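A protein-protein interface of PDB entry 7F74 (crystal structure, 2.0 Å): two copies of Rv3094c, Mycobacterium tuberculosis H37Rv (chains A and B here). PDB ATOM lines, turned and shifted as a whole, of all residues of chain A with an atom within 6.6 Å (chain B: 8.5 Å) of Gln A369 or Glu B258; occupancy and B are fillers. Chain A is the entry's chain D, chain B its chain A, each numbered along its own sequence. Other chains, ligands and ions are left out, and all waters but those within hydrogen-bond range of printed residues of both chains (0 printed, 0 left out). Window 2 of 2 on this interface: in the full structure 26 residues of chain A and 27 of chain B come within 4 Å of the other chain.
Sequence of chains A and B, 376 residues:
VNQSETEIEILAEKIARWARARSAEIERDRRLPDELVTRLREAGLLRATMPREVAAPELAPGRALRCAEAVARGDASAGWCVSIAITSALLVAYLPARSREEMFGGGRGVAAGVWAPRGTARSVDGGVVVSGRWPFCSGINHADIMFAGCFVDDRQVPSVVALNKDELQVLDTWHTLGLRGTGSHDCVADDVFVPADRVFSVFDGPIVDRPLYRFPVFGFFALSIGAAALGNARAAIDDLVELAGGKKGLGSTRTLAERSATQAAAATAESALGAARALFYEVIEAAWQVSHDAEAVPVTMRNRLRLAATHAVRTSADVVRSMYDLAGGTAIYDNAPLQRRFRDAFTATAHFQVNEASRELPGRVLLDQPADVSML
Of the 19 printed residues of chain B, 5 touch a printed residue of chain A.
Hydrophobic or aromatic side chains of chain B that line the printed part of chain A: Val B241 and Ala B257.
Hydrophobic or aromatic side chains of chain A within 4 Å of the printed part of chain B: Leu A367.
Among the printed residues, 8 pairs touch across the chains.
The guanidinium group (NH1) of Arg A364 sits at hydrogen-bond distance from the side-chain amide oxygen (OE1) of Gln B263 (3.1 Å).
Among the printed residues, merely in contact across the chains: Gly A363 with Gln B263 (3.2 Å), Gln A369 with Glu B258 (3.2 Å), Gln A369 with Ala B257 (3.3 Å), Leu A367 with Gln B263 (3.7 Å), Leu A366 with Val B241 (3.7 Å), Leu A367 with Thr B262 (3.8 Å) and Leu A367 with Ala B257 (3.9 Å).
The backbone carbonyl oxygen (O) of Ala B244 lies close to the backbone NH (N) of Ala B257 (3.1 Å).
N of Thr B255 sits at hydrogen-bond distance from OE1 of Glu B258.
O of Leu B256 sits at hydrogen-bond distance from OG1 of Thr B262 (2.8 Å).
The backbone carbonyl oxygen (O) of Ala B257 is in hydrogen-bond range of the side-chain amide nitrogen (NE2) of Gln B263 (2.9 Å).
The backbone carbonyl oxygen of Arg A364 is in hydrogen-bond range of the backbone NH of Gln A369.
O of Leu A367 sits at hydrogen-bond distance from NE2 of Gln A369, at 3.0 Å.
No position is printed for both chains.
Of the 8 pairs that touch across the chains among the printed residues, none has its exchanged pair printed and touching as well.
Of the printed residues of chain B, Gly A363 touches Gln B263.
Of the printed residues of chain B, Gln A369 touches Ala B257 (3.3 Å) and Glu B258 (3.2 Å).
No residue of chain B comes within 4 Å of Pro A370.
Glu B258 touches one residue of chain A.
Printed residues of chain A within 4 Å of Thr B262: Leu A367.
The nearest printed residue of chain B that does not touch Gln A369 is Thr B255 (4.01 Å).
The nearest printed residue of chain A that does not touch Ala B257 is Arg A364 (5.4 Å).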
ATOM      1  N   GLY A 363      13.060 -20.741  28.534  1.00  0.00           N
ATOM      2  CA  GLY A 363      14.405 -20.715  27.963  1.00  0.00           C
ATOM      3  C   GLY A 363      15.370 -19.867  28.775  1.00  0.00           C
ATOM      4  O   GLY A 363      16.506 -20.282  29.039  1.00  0.00           O
ATOM      5  N   ARG A 364      14.927 -18.671  29.193  1.00  0.00           N
ATOM      6  CA  ARG A 364      15.784 -17.805  30.000  1.00  0.00           C
ATOM      7  C   ARG A 364      16.193 -18.502  31.287  1.00  0.00           C
ATOM      8  O   ARG A 364      17.332 -18.363  31.740  1.00  0.00           O
ATOM      9  CB  ARG A 364      15.078 -16.475  30.306  1.00  0.00           C
ATOM     10  CG  ARG A 364      15.245 -15.405  29.235  1.00  0.00           C
ATOM     11  CD  ARG A 364      14.873 -13.953  29.701  1.00  0.00           C
ATOM     12  NE  ARG A 364      13.451 -13.799  30.017  1.00  0.00           N
ATOM     13  CZ  ARG A 364      12.445 -13.840  29.128  1.00  0.00           C
ATOM     14  NH1 ARG A 364      12.694 -14.031  27.834  1.00  0.00           N
ATOM     15  NH2 ARG A 364      11.182 -13.680  29.526  1.00  0.00           N
ATOM     16  N   VAL A 365      15.276 -19.258  31.894  1.00  0.00           N
ATOM     17  CA  VAL A 365      15.608 -20.000  33.103  1.00  0.00           C
ATOM     18  C   VAL A 365      16.614 -21.100  32.795  1.00  0.00           C
ATOM     19  O   VAL A 365      17.533 -21.357  33.585  1.00  0.00           O
ATOM     20  CB  VAL A 365      14.342 -20.576  33.765  1.00  0.00           C
ATOM     21  CG1 VAL A 365      14.744 -21.572  34.862  1.00  0.00           C
ATOM     22  CG2 VAL A 365      13.484 -19.458  34.331  1.00  0.00           C
ATOM     23  N   LEU A 366      16.447 -21.792  31.666  1.00  0.00           N
ATOM     24  CA  LEU A 366      17.400 -22.842  31.308  1.00  0.00           C
ATOM     25  C   LEU A 366      18.795 -22.257  31.073  1.00  0.00           C
ATOM     26  O   LEU A 366      19.811 -22.860  31.454  1.00  0.00           O
ATOM     27  CB  LEU A 366      16.913 -23.588  30.067  1.00  0.00           C
ATOM     28  CG  LEU A 366      15.737 -24.556  30.173  1.00  0.00           C
ATOM     29  CD1 LEU A 366      15.206 -24.830  28.746  1.00  0.00           C
ATOM     30  CD2 LEU A 366      16.174 -25.848  30.898  1.00  0.00           C
ATOM     31  N   LEU A 367      18.873 -21.094  30.448  1.00  0.00           N
ATOM     32  CA  LEU A 367      20.181 -20.494  30.163  1.00  0.00           C
ATOM     33  C   LEU A 367      20.726 -19.682  31.338  1.00  0.00           C
ATOM     34  O   LEU A 367      21.721 -18.973  31.174  1.00  0.00           O
ATOM     35  CB  LEU A 367      20.106 -19.630  28.899  1.00  0.00           C
ATOM     36  CG  LEU A 367      19.652 -20.395  27.640  1.00  0.00           C
ATOM     37  CD1 LEU A 367      19.100 -19.485  26.545  1.00  0.00           C
ATOM     38  CD2 LEU A 367      20.763 -21.269  27.058  1.00  0.00           C
ATOM     39  N   ASP A 368      20.119 -19.806  32.518  1.00  0.00           N
ATOM     40  CA  ASP A 368      20.500 -19.062  33.716  1.00  0.00           C
ATOM     41  C   ASP A 368      20.751 -17.587  33.405  1.00  0.00           C
ATOM     42  O   ASP A 368      21.808 -17.020  33.694  1.00  0.00           O
ATOM     43  CB  ASP A 368      21.721 -19.691  34.394  1.00  0.00           C
ATOM     44  CG  ASP A 368      21.977 -19.113  35.762  1.00  0.00           C
ATOM     45  OD1 ASP A 368      21.155 -19.353  36.676  1.00  0.00           O
ATOM     46  OD2 ASP A 368      22.985 -18.399  35.911  1.00  0.00           O
ATOM     47  N   GLN A 369      19.726 -16.963  32.822  1.00  0.00           N
ATOM     48  CA  GLN A 369      19.636 -15.537  32.570  1.00  0.00           C
ATOM     49  C   GLN A 369      18.675 -14.879  33.560  1.00  0.00           C
ATOM     50  O   GLN A 369      17.708 -15.508  34.018  1.00  0.00           O
ATOM     51  CB  GLN A 369      19.156 -15.276  31.136  1.00  0.00           C
ATOM     52  CG  GLN A 369      20.082 -15.893  30.052  1.00  0.00           C
ATOM     53  CD  GLN A 369      21.488 -15.305  30.068  1.00  0.00           C
ATOM     54  OE1 GLN A 369      21.674 -14.128  29.768  1.00  0.00           O
ATOM     55  NE2 GLN A 369      22.483 -16.128  30.413  1.00  0.00           N
ATOM     56  N   PRO A 370      18.911 -13.619  33.931  1.00  0.00           N
ATOM     57  CA  PRO A 370      17.912 -12.908  34.742  1.00  0.00           C
ATOM     58  C   PRO A 370      16.522 -13.115  34.170  1.00  0.00           C
ATOM     59  O   PRO A 370      16.300 -13.014  32.959  1.00  0.00           O
ATOM     60  CB  PRO A 370      18.348 -11.440  34.657  1.00  0.00           C
ATOM     61  CG  PRO A 370      19.825 -11.497  34.352  1.00  0.00           C
ATOM     62  CD  PRO A 370      20.083 -12.776  33.592  1.00  0.00           C
ATOM     63  N   ALA A 371      15.577 -13.412  35.048  1.00  0.00           N
ATOM     64  CA  ALA A 371      14.209 -13.600  34.608  1.00  0.00           C
ATOM     65  C   ALA A 371      13.266 -13.250  35.747  1.00  0.00           C
ATOM     66  O   ALA A 371      13.561 -13.504  36.922  1.00  0.00           O
ATOM     67  CB  ALA A 371      13.986 -15.044  34.132  1.00  0.00           C
ATOM     68  N   ASP A 372      12.145 -12.639  35.384  1.00  0.00           N
ATOM     69  CA  ASP A 372      11.021 -12.441  36.291  1.00  0.00           C
ATOM     70  C   ASP A 372      10.165 -13.708  36.233  1.00  0.00           C
ATOM     71  O   ASP A 372       9.399 -13.915  35.284  1.00  0.00           O
ATOM     72  CB  ASP A 372      10.255 -11.186  35.888  1.00  0.00           C
ATOM     73  CG  ASP A 372       8.942 -11.034  36.627  1.00  0.00           C
ATOM     74  OD1 ASP A 372       8.788 -11.622  37.726  1.00  0.00           O
ATOM     75  OD2 ASP A 372       8.081 -10.286  36.111  1.00  0.00           O
ATOM     76  N   VAL B 241      24.429 -24.728  26.511  1.00  0.00           N
ATOM     77  CA  VAL B 241      24.078 -23.857  27.628  1.00  0.00           C
ATOM     78  C   VAL B 241      25.344 -23.262  28.228  1.00  0.00           C
ATOM     79  O   VAL B 241      25.408 -22.064  28.527  1.00  0.00           O
ATOM     80  CB  VAL B 241      23.253 -24.622  28.674  1.00  0.00           C
ATOM     81  CG1 VAL B 241      23.127 -23.754  29.960  1.00  0.00           C
ATOM     82  CG2 VAL B 241      21.908 -24.987  28.102  1.00  0.00           C
ATOM     83  N   LEU B 243      28.243 -22.731  26.651  1.00  0.00           N
ATOM     84  CA  LEU B 243      28.798 -21.736  25.749  1.00  0.00           C
ATOM     85  C   LEU B 243      27.988 -20.442  25.771  1.00  0.00           C
ATOM     86  O   LEU B 243      28.546 -19.351  25.633  1.00  0.00           O
ATOM     87  CB  LEU B 243      28.866 -22.308  24.325  1.00  0.00           C
ATOM     88  CG  LEU B 243      29.204 -21.314  23.218  1.00  0.00           C
ATOM     89  CD1 LEU B 243      30.752 -21.036  23.224  1.00  0.00           C
ATOM     90  CD2 LEU B 243      28.737 -21.766  21.844  1.00  0.00           C
ATOM     91  N   ALA B 244      26.665 -20.534  25.895  1.00  0.00           N
ATOM     92  CA  ALA B 244      25.820 -19.379  25.595  1.00  0.00           C
ATOM     93  C   ALA B 244      25.807 -18.359  26.724  1.00  0.00           C
ATOM     94  O   ALA B 244      25.519 -17.179  26.470  1.00  0.00           O
ATOM     95  CB  ALA B 244      24.375 -19.805  25.266  1.00  0.00           C
ATOM     96  N   GLY B 245      26.141 -18.769  27.944  1.00  0.00           N
ATOM     97  CA  GLY B 245      26.268 -17.802  29.018  1.00  0.00           C
ATOM     98  C   GLY B 245      27.276 -16.710  28.705  1.00  0.00           C
ATOM     99  O   GLY B 245      27.042 -15.530  29.004  1.00  0.00           O
ATOM    100  N   GLY B 246      28.398 -17.077  28.062  1.00  0.00           N
ATOM    101  CA  GLY B 246      29.485 -16.137  27.840  1.00  0.00           C
ATOM    102  C   GLY B 246      29.890 -15.791  26.415  1.00  0.00           C
ATOM    103  O   GLY B 246      30.940 -15.173  26.224  1.00  0.00           O
ATOM    104  N   LYS B 247      29.084 -16.144  25.412  1.00  0.00           N
ATOM    105  CA  LYS B 247      29.425 -15.857  24.015  1.00  0.00           C
ATOM    106  C   LYS B 247      28.827 -14.516  23.576  1.00  0.00           C
ATOM    107  O   LYS B 247      27.639 -14.425  23.253  1.00  0.00           O
ATOM    108  CB  LYS B 247      28.953 -16.978  23.087  1.00  0.00           C
ATOM    109  CG  LYS B 247      29.226 -16.665  21.610  1.00  0.00           C
ATOM    110  CD  LYS B 247      29.401 -17.877  20.703  1.00  0.00           C
ATOM    111  CE  LYS B 247      29.579 -17.389  19.243  1.00  0.00           C
ATOM    112  NZ  LYS B 247      29.430 -18.448  18.206  1.00  0.00           N
ATOM    113  N   LYS B 248      29.663 -13.478  23.514  1.00  0.00           N
ATOM    114  CA  LYS B 248      29.265 -12.164  23.017  1.00  0.00           C
ATOM    115  C   LYS B 248      29.964 -11.906  21.684  1.00  0.00           C
ATOM    116  O   LYS B 248      31.184 -12.081  21.569  1.00  0.00           O
ATOM    117  CB  LYS B 248      29.603 -11.058  24.035  1.00  0.00           C
ATOM    118  CG  LYS B 248      29.155  -9.628  23.638  1.00  0.00           C
ATOM    119  CD  LYS B 248      29.481  -8.553  24.715  1.00  0.00           C
ATOM    120  CE  LYS B 248      28.562  -8.564  25.956  1.00  0.00           C
ATOM    121  NZ  LYS B 248      27.179  -8.078  25.666  1.00  0.00           N
ATOM    122  N   SER B 252      27.200  -7.083  19.176  1.00  0.00           N
ATOM    123  CA  SER B 252      25.992  -7.846  19.455  1.00  0.00           C
ATOM    124  C   SER B 252      25.159  -7.297  20.609  1.00  0.00           C
ATOM    125  O   SER B 252      23.998  -7.708  20.753  1.00  0.00           O
ATOM    126  CB  SER B 252      26.374  -9.316  19.727  1.00  0.00           C
ATOM    127  OG  SER B 252      26.970  -9.497  21.005  1.00  0.00           O
ATOM    128  N   THR B 253      25.704  -6.371  21.411  1.00  0.00           N
ATOM    129  CA  THR B 253      25.040  -5.781  22.577  1.00  0.00           C
ATOM    130  C   THR B 253      24.338  -6.834  23.434  1.00  0.00           C
ATOM    131  O   THR B 253      23.411  -6.514  24.189  1.00  0.00           O
ATOM    132  CB  THR B 253      24.058  -4.677  22.134  1.00  0.00           C
ATOM    133  OG1 THR B 253      23.738  -3.839  23.256  1.00  0.00           O
ATOM    134  CG2 THR B 253      22.761  -5.243  21.536  1.00  0.00           C
ATOM    135  N   ARG B 254      24.818  -8.077  23.363  1.00  0.00           N
ATOM    136  CA  ARG B 254      24.155  -9.218  23.978  1.00  0.00           C
ATOM    137  C   ARG B 254      25.138 -10.379  24.073  1.00  0.00           C
ATOM    138  O   ARG B 254      26.111 -10.459  23.319  1.00  0.00           O
ATOM    139  CB  ARG B 254      22.954  -9.693  23.150  1.00  0.00           C
ATOM    140  CG  ARG B 254      21.673  -8.899  23.239  1.00  0.00           C
ATOM    141  CD  ARG B 254      20.996  -9.005  21.878  1.00  0.00           C
ATOM    142  NE  ARG B 254      19.595  -8.611  21.888  1.00  0.00           N
ATOM    143  CZ  ARG B 254      18.804  -8.671  20.820  1.00  0.00           C
ATOM    144  NH1 ARG B 254      19.283  -9.104  19.656  1.00  0.00           N
ATOM    145  NH2 ARG B 254      17.533  -8.296  20.915  1.00  0.00           N
ATOM    146  N   THR B 255      24.843 -11.312  24.968  1.00  0.00           N
ATOM    147  CA  THR B 255      25.390 -12.650  24.805  1.00  0.00           C
ATOM    148  C   THR B 255      24.462 -13.450  23.875  1.00  0.00           C
ATOM    149  O   THR B 255      23.386 -12.990  23.471  1.00  0.00           O
ATOM    150  CB  THR B 255      25.582 -13.348  26.160  1.00  0.00           C
ATOM    151  OG1 THR B 255      24.355 -13.353  26.895  1.00  0.00           O
ATOM    152  CG2 THR B 255      26.684 -12.651  26.985  1.00  0.00           C
ATOM    153  N   LEU B 256      24.918 -14.648  23.493  1.00  0.00           N
ATOM    154  CA  LEU B 256      24.049 -15.576  22.773  1.00  0.00           C
ATOM    155  C   LEU B 256      22.837 -15.948  23.622  1.00  0.00           C
ATOM    156  O   LEU B 256      21.719 -16.065  23.105  1.00  0.00           O
ATOM    157  CB  LEU B 256      24.841 -16.825  22.386  1.00  0.00           C
ATOM    158  CG  LEU B 256      24.170 -17.935  21.582  1.00  0.00           C
ATOM    159  CD1 LEU B 256      23.531 -17.380  20.333  1.00  0.00           C
ATOM    160  CD2 LEU B 256      25.210 -18.990  21.195  1.00  0.00           C
ATOM    161  N   ALA B 257      23.038 -16.089  24.939  1.00  0.00           N
ATOM    162  CA  ALA B 257      21.956 -16.475  25.838  1.00  0.00           C
ATOM    163  C   ALA B 257      20.899 -15.378  25.985  1.00  0.00           C
ATOM    164  O   ALA B 257      19.731 -15.689  26.274  1.00  0.00           O
ATOM    165  CB  ALA B 257      22.523 -16.852  27.210  1.00  0.00           C
ATOM    166  N   GLU B 258      21.276 -14.105  25.786  1.00  0.00           N
ATOM    167  CA  GLU B 258      20.340 -12.986  25.924  1.00  0.00           C
ATOM    168  C   GLU B 258      19.457 -12.764  24.689  1.00  0.00           C
ATOM    169  O   GLU B 258      18.680 -11.802  24.658  1.00  0.00           O
ATOM    170  CB  GLU B 258      21.103 -11.699  26.253  1.00  0.00           C
ATOM    171  CG  GLU B 258      21.555 -11.634  27.727  1.00  0.00           C
ATOM    172  CD  GLU B 258      22.673 -10.645  27.966  1.00  0.00           C
ATOM    173  OE1 GLU B 258      23.135 -10.013  26.991  1.00  0.00           O
ATOM    174  OE2 GLU B 258      23.082 -10.501  29.139  1.00  0.00           O
ATOM    175  N   ARG B 259      19.529 -13.626  23.680  1.00  0.00           N
ATOM    176  CA  ARG B 259      18.669 -13.504  22.509  1.00  0.00           C
ATOM    177  C   ARG B 259      17.413 -14.369  22.646  1.00  0.00           C
ATOM    178  O   ARG B 259      17.471 -15.522  23.102  1.00  0.00           O
ATOM    179  CB  ARG B 259      19.444 -13.862  21.240  1.00  0.00           C
ATOM    180  CG  ARG B 259      20.535 -12.812  20.883  1.00  0.00           C
ATOM    181  CD  ARG B 259      21.380 -13.179  19.652  1.00  0.00           C
ATOM    182  NE  ARG B 259      20.661 -13.999  18.671  1.00  0.00           N
ATOM    183  CZ  ARG B 259      19.673 -13.569  17.873  1.00  0.00           C
ATOM    184  NH1 ARG B 259      19.280 -12.291  17.884  1.00  0.00           N
ATOM    185  NH2 ARG B 259      19.079 -14.429  17.042  1.00  0.00           N
ATOM    186  N   SER B 260      16.267 -13.781  22.281  1.00  0.00           N
ATOM    187  CA  SER B 260      14.996 -14.476  22.440  1.00  0.00           C
ATOM    188  C   SER B 260      15.010 -15.808  21.702  1.00  0.00           C
ATOM    189  O   SER B 260      14.472 -16.805  22.195  1.00  0.00           O
ATOM    190  CB  SER B 260      13.843 -13.616  21.918  1.00  0.00           C
ATOM    191  OG  SER B 260      13.794 -12.403  22.614  1.00  0.00           O
ATOM    192  N   ALA B 261      15.576 -15.823  20.487  1.00  0.00           N
ATOM    193  CA  ALA B 261      15.584 -17.038  19.684  1.00  0.00           C
ATOM    194  C   ALA B 261      16.360 -18.155  20.379  1.00  0.00           C
ATOM    195  O   ALA B 261      15.987 -19.335  20.289  1.00  0.00           O
ATOM    196  CB  ALA B 261      16.177 -16.730  18.306  1.00  0.00           C
ATOM    197  N   THR B 262      17.468 -17.804  21.042  1.00  0.00           N
ATOM    198  CA  THR B 262      18.256 -18.819  21.722  1.00  0.00           C
ATOM    199  C   THR B 262      17.426 -19.426  22.828  1.00  0.00           C
ATOM    200  O   THR B 262      17.411 -20.650  23.014  1.00  0.00           O
ATOM    201  CB  THR B 262      19.543 -18.224  22.310  1.00  0.00           C
ATOM    202  OG1 THR B 262      20.318 -17.597  21.279  1.00  0.00           O
ATOM    203  CG2 THR B 262      20.359 -19.294  23.006  1.00  0.00           C
ATOM    204  N   GLN B 263      16.729 -18.569  23.572  1.00  0.00           N
ATOM    205  CA  GLN B 263      15.931 -19.024  24.714  1.00  0.00           C
ATOM    206  C   GLN B 263      14.804 -19.932  24.258  1.00  0.00           C
ATOM    207  O   GLN B 263      14.610 -21.033  24.802  1.00  0.00           O
ATOM    208  CB  GLN B 263      15.384 -17.814  25.485  1.00  0.00           C
ATOM    209  CG  GLN B 263      16.516 -16.923  26.071  1.00  0.00           C
ATOM    210  CD  GLN B 263      16.129 -15.457  26.232  1.00  0.00           C
ATOM    211  OE1 GLN B 263      14.985 -15.081  26.033  1.00  0.00           O
ATOM    212  NE2 GLN B 263      17.084 -14.637  26.626  1.00  0.00           N
